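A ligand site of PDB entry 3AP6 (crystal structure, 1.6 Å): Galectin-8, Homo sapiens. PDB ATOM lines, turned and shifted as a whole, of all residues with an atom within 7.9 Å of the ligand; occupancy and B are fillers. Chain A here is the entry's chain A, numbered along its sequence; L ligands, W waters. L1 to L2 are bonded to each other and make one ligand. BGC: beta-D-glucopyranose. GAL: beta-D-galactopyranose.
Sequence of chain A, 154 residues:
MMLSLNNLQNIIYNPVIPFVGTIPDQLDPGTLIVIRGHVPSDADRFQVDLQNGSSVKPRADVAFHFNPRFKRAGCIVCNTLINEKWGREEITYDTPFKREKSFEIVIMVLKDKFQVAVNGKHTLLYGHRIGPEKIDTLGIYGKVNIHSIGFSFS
Water W1 lies within hydrogen-bond range of OE1 of Glu 89 (2.7 Å) and O2 of BGC L1 (2.7 Å).
Water W2 bridges an oxygen (O6) of BGC L1 and the side-chain carboxylate (OE2) of Glu 89.
N of His 65 is in hydrogen-bond range of O of Asn 79, at 2.9 Å.
O of Gly 87 lies within hydrogen-bond range of ND2 of Asn 79 (3.0 Å).
The side-chain amide oxygen (OD1) of Asn 79 lies close to the backbone carbonyl oxygen (O) of Arg 88, 3.3 Å away.
NE of Arg 69 lies close to ND2 of Asn 67.
NE2 of His 65 sits close to ND2 of Asn 67, at 3.4 Å.
The guanidinium group (NH1) of Arg 45 lies close to the side-chain amide nitrogen (ND2) of Asn 67 (3.4 Å).
NH2 of Arg 45 is in hydrogen-bond range of OE1 of Gln 47 (2.8 Å).
The side-chain amide oxygen of Asn 67 sits close to the backbone carbonyl oxygen of Phe 46 (2.7 Å).
Residues that only touch the ligand: Trp 86.
Hydrophobic or aromatic side chains that line the ligand: His 65 and Trp 86.
Within 4 Å of the ligand: Arg 45, His 65, Asn 67, Arg 69, Asn 79, Trp 86 and Glu 89.
Along chain A the residues within 4 Å of the ligand span positions 45 to 89.
The side-chain carboxylate of Glu 89 is in hydrogen-bond range of an oxygen (O3) of BGC L1 (2.6 Å).
O6 of GAL L2 lies within hydrogen-bond range of ND2 of Asn 79 (2.8 Å).
NH1 of Arg 69 lies within hydrogen-bond range of O3 of BGC L1 (2.9 Å).
An oxygen (O4) of GAL L2 is in hydrogen-bond range of a ring nitrogen (NE2) of His 65, 2.9 Å away.
The guanidinium group of Arg 45 lies within hydrogen-bond range of an oxygen (O4) of GAL L2 (3.1 Å).
The side-chain amide nitrogen (ND2) of Asn 67 sits at hydrogen-bond distance from an oxygen (O4) of GAL L2, at 3.2 Å.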
ATOM      1  N   ARG A  45      17.512 -23.658 -13.981  1.00  0.00           N
ATOM      2  CA  ARG A  45      16.288 -23.405 -14.762  1.00  0.00           C
ATOM      3  C   ARG A  45      15.236 -22.787 -13.873  1.00  0.00           C
ATOM      4  O   ARG A  45      15.289 -22.892 -12.655  1.00  0.00           O
ATOM      5  CB  ARG A  45      15.757 -24.705 -15.352  1.00  0.00           C
ATOM      6  CG  ARG A  45      15.498 -25.781 -14.303  1.00  0.00           C
ATOM      7  CD  ARG A  45      14.746 -26.950 -14.923  1.00  0.00           C
ATOM      8  NE  ARG A  45      13.299 -26.700 -14.984  1.00  0.00           N
ATOM      9  CZ  ARG A  45      12.447 -27.389 -15.752  1.00  0.00           C
ATOM     10  NH1 ARG A  45      12.893 -28.331 -16.578  1.00  0.00           N
ATOM     11  NH2 ARG A  45      11.145 -27.118 -15.694  1.00  0.00           N
ATOM     12  N   PHE A  46      14.263 -22.117 -14.485  1.00  0.00           N
ATOM     13  CA  PHE A  46      13.062 -21.765 -13.769  1.00  0.00           C
ATOM     14  C   PHE A  46      11.941 -21.822 -14.780  1.00  0.00           C
ATOM     15  O   PHE A  46      12.196 -22.039 -15.960  1.00  0.00           O
ATOM     16  CB  PHE A  46      13.155 -20.396 -13.073  1.00  0.00           C
ATOM     17  CG  PHE A  46      13.097 -19.190 -14.005  1.00  0.00           C
ATOM     18  CD1 PHE A  46      11.881 -18.581 -14.300  1.00  0.00           C
ATOM     19  CD2 PHE A  46      14.257 -18.629 -14.504  1.00  0.00           C
ATOM     20  CE1 PHE A  46      11.841 -17.453 -15.140  1.00  0.00           C
ATOM     21  CE2 PHE A  46      14.231 -17.503 -15.335  1.00  0.00           C
ATOM     22  CZ  PHE A  46      13.029 -16.918 -15.663  1.00  0.00           C
ATOM     23  N   GLN A  47      10.716 -21.663 -14.318  1.00  0.00           N
ATOM     24  CA  GLN A  47       9.586 -21.696 -15.244  1.00  0.00           C
ATOM     25  C   GLN A  47       8.435 -20.813 -14.802  1.00  0.00           C
ATOM     26  O   GLN A  47       8.198 -20.590 -13.606  1.00  0.00           O
ATOM     27  CB  GLN A  47       9.084 -23.125 -15.428  1.00  0.00           C
ATOM     28  CG  GLN A  47       8.309 -23.671 -14.246  1.00  0.00           C
ATOM     29  CD  GLN A  47       8.447 -25.157 -14.133  1.00  0.00           C
ATOM     30  OE1 GLN A  47       9.551 -25.663 -13.875  1.00  0.00           O
ATOM     31  NE2 GLN A  47       7.348 -25.893 -14.379  1.00  0.00           N
ATOM     32  N   ASP A  49       4.405 -20.897 -15.622  1.00  0.00           N
ATOM     33  CA  ASP A  49       3.362 -21.804 -16.137  1.00  0.00           C
ATOM     34  C   ASP A  49       1.977 -21.142 -16.029  1.00  0.00           C
ATOM     35  O   ASP A  49       1.560 -20.715 -14.937  1.00  0.00           O
ATOM     36  CB  ASP A  49       3.339 -23.113 -15.319  1.00  0.00           C
ATOM     37  CG  ASP A  49       4.581 -23.998 -15.515  1.00  0.00           C
ATOM     38  OD1 ASP A  49       5.338 -23.779 -16.482  1.00  0.00           O
ATOM     39  OD2 ASP A  49       4.798 -24.906 -14.680  1.00  0.00           O
ATOM     40  N   ARG A  59      -1.569 -33.736 -11.725  1.00  0.00           N
ATOM     41  CA  ARG A  59      -0.957 -32.434 -11.985  1.00  0.00           C
ATOM     42  C   ARG A  59      -1.873 -31.609 -12.902  1.00  0.00           C
ATOM     43  O   ARG A  59      -2.411 -32.131 -13.871  1.00  0.00           O
ATOM     44  CB  ARG A  59       0.417 -32.601 -12.620  1.00  0.00           C
ATOM     45  CG  ARG A  59       1.172 -31.304 -12.743  1.00  0.00           C
ATOM     46  CD  ARG A  59       2.568 -31.541 -13.244  1.00  0.00           C
ATOM     47  NE  ARG A  59       3.259 -30.284 -13.521  1.00  0.00           N
ATOM     48  CZ  ARG A  59       4.496 -30.199 -14.008  1.00  0.00           C
ATOM     49  NH1 ARG A  59       5.192 -31.291 -14.271  1.00  0.00           N
ATOM     50  NH2 ARG A  59       5.028 -29.012 -14.238  1.00  0.00           N
ATOM     51  N   HIS A  65       3.877 -23.472 -20.746  1.00  0.00           N
ATOM     52  CA  HIS A  65       5.117 -23.646 -19.954  1.00  0.00           C
ATOM     53  C   HIS A  65       6.224 -22.863 -20.657  1.00  0.00           C
ATOM     54  O   HIS A  65       6.558 -23.152 -21.799  1.00  0.00           O
ATOM     55  CB  HIS A  65       5.419 -25.133 -19.945  1.00  0.00           C
ATOM     56  CG  HIS A  65       6.694 -25.559 -19.280  1.00  0.00           C
ATOM     57  ND1 HIS A  65       6.889 -25.541 -17.913  1.00  0.00           N
ATOM     58  CD2 HIS A  65       7.797 -26.143 -19.814  1.00  0.00           C
ATOM     59  CE1 HIS A  65       8.084 -26.052 -17.642  1.00  0.00           C
ATOM     60  NE2 HIS A  65       8.651 -26.407 -18.779  1.00  0.00           N
ATOM     61  N   PHE A  66       6.756 -21.887 -19.927  1.00  0.00           N
ATOM     62  CA  PHE A  66       7.807 -20.998 -20.399  1.00  0.00           C
ATOM     63  C   PHE A  66       9.018 -21.223 -19.518  1.00  0.00           C
ATOM     64  O   PHE A  66       9.038 -20.859 -18.373  1.00  0.00           O
ATOM     65  CB  PHE A  66       7.318 -19.567 -20.360  1.00  0.00           C
ATOM     66  CG  PHE A  66       8.343 -18.555 -20.758  1.00  0.00           C
ATOM     67  CD1 PHE A  66       8.497 -18.196 -22.086  1.00  0.00           C
ATOM     68  CD2 PHE A  66       9.131 -17.921 -19.797  1.00  0.00           C
ATOM     69  CE1 PHE A  66       9.419 -17.245 -22.473  1.00  0.00           C
ATOM     70  CE2 PHE A  66      10.062 -16.967 -20.195  1.00  0.00           C
ATOM     71  CZ  PHE A  66      10.200 -16.632 -21.515  1.00  0.00           C
ATOM     72  N   ASN A  67      10.041 -21.877 -20.062  1.00  0.00           N
ATOM     73  CA  ASN A  67      11.048 -22.508 -19.217  1.00  0.00           C
ATOM     74  C   ASN A  67      12.481 -22.203 -19.649  1.00  0.00           C
ATOM     75  O   ASN A  67      13.105 -22.995 -20.408  1.00  0.00           O
ATOM     76  CB  ASN A  67      10.808 -24.023 -19.260  1.00  0.00           C
ATOM     77  CG  ASN A  67      11.827 -24.813 -18.465  1.00  0.00           C
ATOM     78  OD1 ASN A  67      12.357 -24.358 -17.420  1.00  0.00           O
ATOM     79  ND2 ASN A  67      12.073 -26.018 -18.919  1.00  0.00           N
ATOM     80  N   ARG A  69      16.378 -22.248 -19.509  1.00  0.00           N
ATOM     81  CA  ARG A  69      17.383 -23.185 -18.983  1.00  0.00           C
ATOM     82  C   ARG A  69      18.772 -22.603 -19.242  1.00  0.00           C
ATOM     83  O   ARG A  69      18.989 -21.977 -20.261  1.00  0.00           O
ATOM     84  CB  ARG A  69      17.227 -24.547 -19.642  1.00  0.00           C
ATOM     85  CG  ARG A  69      15.841 -25.186 -19.454  1.00  0.00           C
ATOM     86  CD  ARG A  69      15.770 -26.571 -20.036  1.00  0.00           C
ATOM     87  NE  ARG A  69      14.467 -27.193 -19.842  1.00  0.00           N
ATOM     88  CZ  ARG A  69      14.099 -28.366 -20.358  1.00  0.00           C
ATOM     89  NH1 ARG A  69      14.944 -29.056 -21.107  1.00  0.00           N
ATOM     90  NH2 ARG A  69      12.871 -28.841 -20.143  1.00  0.00           N
ATOM     91  N   VAL A  77      12.704 -23.426 -23.302  1.00  0.00           N
ATOM     92  CA  VAL A  77      11.836 -24.538 -23.727  1.00  0.00           C
ATOM     93  C   VAL A  77      10.387 -24.157 -23.452  1.00  0.00           C
ATOM     94  O   VAL A  77      10.045 -23.815 -22.319  1.00  0.00           O
ATOM     95  CB  VAL A  77      12.151 -25.819 -22.941  1.00  0.00           C
ATOM     96  CG1 VAL A  77      11.151 -26.933 -23.266  1.00  0.00           C
ATOM     97  CG2 VAL A  77      13.569 -26.278 -23.236  1.00  0.00           C
ATOM     98  N   CYS A  78       9.546 -24.193 -24.497  1.00  0.00           N
ATOM     99  CA  CYS A  78       8.120 -23.959 -24.315  1.00  0.00           C
ATOM    100  C   CYS A  78       7.329 -25.221 -24.635  1.00  0.00           C
ATOM    101  O   CYS A  78       7.661 -25.965 -25.588  1.00  0.00           O
ATOM    102  CB  CYS A  78       7.628 -22.804 -25.186  1.00  0.00           C
ATOM    103  SG  CYS A  78       8.265 -21.168 -24.722  1.00  0.00           S
ATOM    104  N   ASN A  79       6.266 -25.452 -23.882  1.00  0.00           N
ATOM    105  CA  ASN A  79       5.480 -26.668 -24.064  1.00  0.00           C
ATOM    106  C   ASN A  79       4.124 -26.547 -23.364  1.00  0.00           C
ATOM    107  O   ASN A  79       3.765 -25.510 -22.765  1.00  0.00           O
ATOM    108  CB  ASN A  79       6.311 -27.856 -23.530  1.00  0.00           C
ATOM    109  CG  ASN A  79       6.005 -29.190 -24.206  1.00  0.00           C
ATOM    110  OD1 ASN A  79       4.965 -29.239 -25.012  1.00  0.00           O
ATOM    111  ND2 ASN A  79       6.698 -30.194 -23.962  1.00  0.00           N
ATOM    112  N   THR A  80       3.343 -27.624 -23.461  1.00  0.00           N
ATOM    113  CA  THR A  80       2.010 -27.727 -22.916  1.00  0.00           C
ATOM    114  C   THR A  80       1.942 -29.088 -22.250  1.00  0.00           C
ATOM    115  O   THR A  80       2.460 -30.071 -22.820  1.00  0.00           O
ATOM    116  CB  THR A  80       0.981 -27.619 -24.033  1.00  0.00           C
ATOM    117  OG1 THR A  80       0.915 -26.269 -24.530  1.00  0.00           O
ATOM    118  CG2 THR A  80      -0.409 -28.062 -23.575  1.00  0.00           C
ATOM    119  N   LEU A  81       1.334 -29.129 -21.065  1.00  0.00           N
ATOM    120  CA  LEU A  81       1.128 -30.341 -20.295  1.00  0.00           C
ATOM    121  C   LEU A  81      -0.371 -30.638 -20.299  1.00  0.00           C
ATOM    122  O   LEU A  81      -1.164 -29.840 -19.827  1.00  0.00           O
ATOM    123  CB  LEU A  81       1.614 -30.169 -18.856  1.00  0.00           C
ATOM    124  CG  LEU A  81       1.525 -31.412 -17.967  1.00  0.00           C
ATOM    125  CD1 LEU A  81       2.674 -32.349 -18.299  1.00  0.00           C
ATOM    126  CD2 LEU A  81       1.474 -31.068 -16.486  1.00  0.00           C
ATOM    127  N   LYS A  85       0.984 -35.299 -19.293  1.00  0.00           N
ATOM    128  CA  LYS A  85       1.858 -35.714 -20.377  1.00  0.00           C
ATOM    129  C   LYS A  85       2.308 -34.471 -21.169  1.00  0.00           C
ATOM    130  O   LYS A  85       1.465 -33.671 -21.575  1.00  0.00           O
ATOM    131  CB  LYS A  85       1.140 -36.762 -21.237  1.00  0.00           C
ATOM    132  CG  LYS A  85       0.740 -38.013 -20.417  1.00  0.00           C
ATOM    133  CD  LYS A  85      -0.263 -38.928 -21.134  1.00  0.00           C
ATOM    134  CE  LYS A  85      -1.712 -38.624 -20.755  1.00  0.00           C
ATOM    135  NZ  LYS A  85      -2.684 -39.395 -21.578  1.00  0.00           N
ATOM    136  N   TRP A  86       3.620 -34.300 -21.313  1.00  0.00           N
ATOM    137  CA  TRP A  86       4.188 -33.188 -22.091  1.00  0.00           C
ATOM    138  C   TRP A  86       4.040 -33.404 -23.595  1.00  0.00           C
ATOM    139  O   TRP A  86       4.242 -34.518 -24.101  1.00  0.00           O
ATOM    140  CB  TRP A  86       5.680 -32.986 -21.753  1.00  0.00           C
ATOM    141  CG  TRP A  86       5.891 -32.411 -20.392  1.00  0.00           C
ATOM    142  CD1 TRP A  86       6.359 -33.052 -19.278  1.00  0.00           C
ATOM    143  CD2 TRP A  86       5.571 -31.077 -19.983  1.00  0.00           C
ATOM    144  NE1 TRP A  86       6.388 -32.186 -18.209  1.00  0.00           N
ATOM    145  CE2 TRP A  86       5.903 -30.968 -18.619  1.00  0.00           C
ATOM    146  CE3 TRP A  86       5.069 -29.958 -20.651  1.00  0.00           C
ATOM    147  CZ2 TRP A  86       5.722 -29.769 -17.895  1.00  0.00           C
ATOM    148  CZ3 TRP A  86       4.894 -28.769 -19.935  1.00  0.00           C
ATOM    149  CH2 TRP A  86       5.214 -28.688 -18.580  1.00  0.00           C
ATOM    150  N   GLY A  87       3.698 -32.343 -24.322  1.00  0.00           N
ATOM    151  CA  GLY A  87       3.623 -32.383 -25.768  1.00  0.00           C
ATOM    152  C   GLY A  87       4.961 -32.145 -26.425  1.00  0.00           C
ATOM    153  O   GLY A  87       6.020 -32.423 -25.853  1.00  0.00           O
ATOM    154  N   ARG A  88       4.902 -31.608 -27.631  1.00  0.00           N
ATOM    155  CA  ARG A  88       6.087 -31.350 -28.438  1.00  0.00           C
ATOM    156  C   ARG A  88       6.765 -30.035 -28.014  1.00  0.00           C
ATOM    157  O   ARG A  88       6.144 -28.966 -28.033  1.00  0.00           O
ATOM    158  CB  ARG A  88       5.710 -31.268 -29.915  1.00  0.00           C
ATOM    159  CG  ARG A  88       5.690 -32.604 -30.654  1.00  0.00           C
ATOM    160  CD  ARG A  88       4.634 -33.593 -30.171  1.00  0.00           C
ATOM    161  NE  ARG A  88       5.172 -34.964 -30.053  1.00  0.00           N
ATOM    162  CZ  ARG A  88       4.597 -35.958 -29.372  1.00  0.00           C
ATOM    163  NH1 ARG A  88       3.447 -35.781 -28.735  1.00  0.00           N
ATOM    164  NH2 ARG A  88       5.196 -37.152 -29.335  1.00  0.00           N
ATOM    165  N   GLU A  89       8.036 -30.113 -27.649  1.00  0.00           N
ATOM    166  CA  GLU A  89       8.770 -28.937 -27.226  1.00  0.00           C
ATOM    167  C   GLU A  89       9.015 -28.020 -28.400  1.00  0.00           C
ATOM    168  O   GLU A  89       9.281 -28.480 -29.519  1.00  0.00           O
ATOM    169  CB  GLU A  89      10.107 -29.316 -26.580  1.00  0.00           C
ATOM    170  CG  GLU A  89       9.957 -29.995 -25.212  1.00  0.00           C
ATOM    171  CD  GLU A  89      11.271 -30.286 -24.519  1.00  0.00           C
ATOM    172  OE1 GLU A  89      12.328 -30.183 -25.169  1.00  0.00           O
ATOM    173  OE2 GLU A  89      11.237 -30.616 -23.320  1.00  0.00           O
ATOM    174  N   GLU A  90       8.878 -26.720 -28.136  1.00  0.00           N
ATOM    175  CA  GLU A  90       9.343 -25.645 -29.025  1.00  0.00           C
ATOM    176  C   GLU A  90      10.496 -24.929 -28.300  1.00  0.00           C
ATOM    177  O   GLU A  90      10.293 -24.271 -27.273  1.00  0.00           O
ATOM    178  CB  GLU A  90       8.200 -24.665 -29.377  1.00  0.00           C
ATOM    179  CG  GLU A  90       6.950 -25.376 -29.872  1.00  0.00           C
ATOM    180  CD  GLU A  90       5.846 -24.476 -30.329  1.00  0.00           C
ATOM    181  OE1 GLU A  90       6.077 -23.257 -30.469  1.00  0.00           O
ATOM    182  OE2 GLU A  90       4.741 -25.007 -30.553  1.00  0.00           O
ATOM    183  N   ILE A  91      11.715 -25.087 -28.812  1.00  0.00           N
ATOM    184  CA  ILE A  91      12.889 -24.551 -28.155  1.00  0.00           C
ATOM    185  C   ILE A  91      13.431 -23.310 -28.867  1.00  0.00           C
ATOM    186  O   ILE A  91      13.680 -23.338 -30.076  1.00  0.00           O
ATOM    187  CB  ILE A  91      14.014 -25.613 -28.046  1.00  0.00           C
ATOM    188  CG1 ILE A  91      13.496 -26.871 -27.311  1.00  0.00           C
ATOM    189  CG2 ILE A  91      15.232 -25.006 -27.387  1.00  0.00           C
ATOM    190  CD1 ILE A  91      14.469 -28.064 -27.370  1.00  0.00           C
HETATM  191  C2  BGC L   1      13.830 -33.462 -22.719  1.00  0.00           C
HETATM  192  C3  BGC L   1      13.517 -32.643 -21.479  1.00  0.00           C
HETATM  193  C4  BGC L   1      12.298 -33.179 -20.749  1.00  0.00           C
HETATM  194  C5  BGC L   1      12.382 -34.688 -20.548  1.00  0.00           C
HETATM  195  C6  BGC L   1      11.133 -35.274 -19.894  1.00  0.00           C
HETATM  196  C1  BGC L   1      13.862 -34.935 -22.344  1.00  0.00           C
HETATM  197  O1  BGC L   1      14.154 -35.747 -23.488  1.00  0.00           O
HETATM  198  O2  BGC L   1      15.086 -33.061 -23.277  1.00  0.00           O
HETATM  199  O3  BGC L   1      13.305 -31.276 -21.834  1.00  0.00           O
HETATM  200  O4  BGC L   1      12.192 -32.540 -19.477  1.00  0.00           O
HETATM  201  O5  BGC L   1      12.574 -35.284 -21.832  1.00  0.00           O
HETATM  202  O6  BGC L   1       9.962 -34.870 -20.624  1.00  0.00           O
HETATM  203  C1  GAL L   2      10.924 -31.981 -19.154  1.00  0.00           C
HETATM  204  C2  GAL L   2      10.940 -31.527 -17.706  1.00  0.00           C
HETATM  205  C3  GAL L   2       9.709 -30.730 -17.326  1.00  0.00           C
HETATM  206  C4  GAL L   2       9.400 -29.675 -18.381  1.00  0.00           C
HETATM  207  C5  GAL L   2       9.354 -30.357 -19.738  1.00  0.00           C
HETATM  208  C6  GAL L   2       8.952 -29.399 -20.850  1.00  0.00           C
HETATM  209  O2  GAL L   2      10.953 -32.630 -16.805  1.00  0.00           O
HETATM  210  O3  GAL L   2       9.963 -30.105 -16.083  1.00  0.00           O
HETATM  211  O4  GAL L   2      10.403 -28.656 -18.388  1.00  0.00           O
HETATM  212  O5  GAL L   2      10.647 -30.884 -20.051  1.00  0.00           O
HETATM  213  O6  GAL L   2       8.795 -30.158 -22.041  1.00  0.00           O
HETATM  214  O   HOH W   1      14.879 -30.619 -24.418  1.00  0.00           O
HETATM  215  O   HOH W   2       9.033 -33.004 -22.415  1.00  0.00           O
HETATM  216  O   HOH W   3      13.620 -33.652 -16.618  1.00  0.00           O
HETATM  217  O   HOH W   4      12.288 -30.358 -13.669  1.00  0.00           O
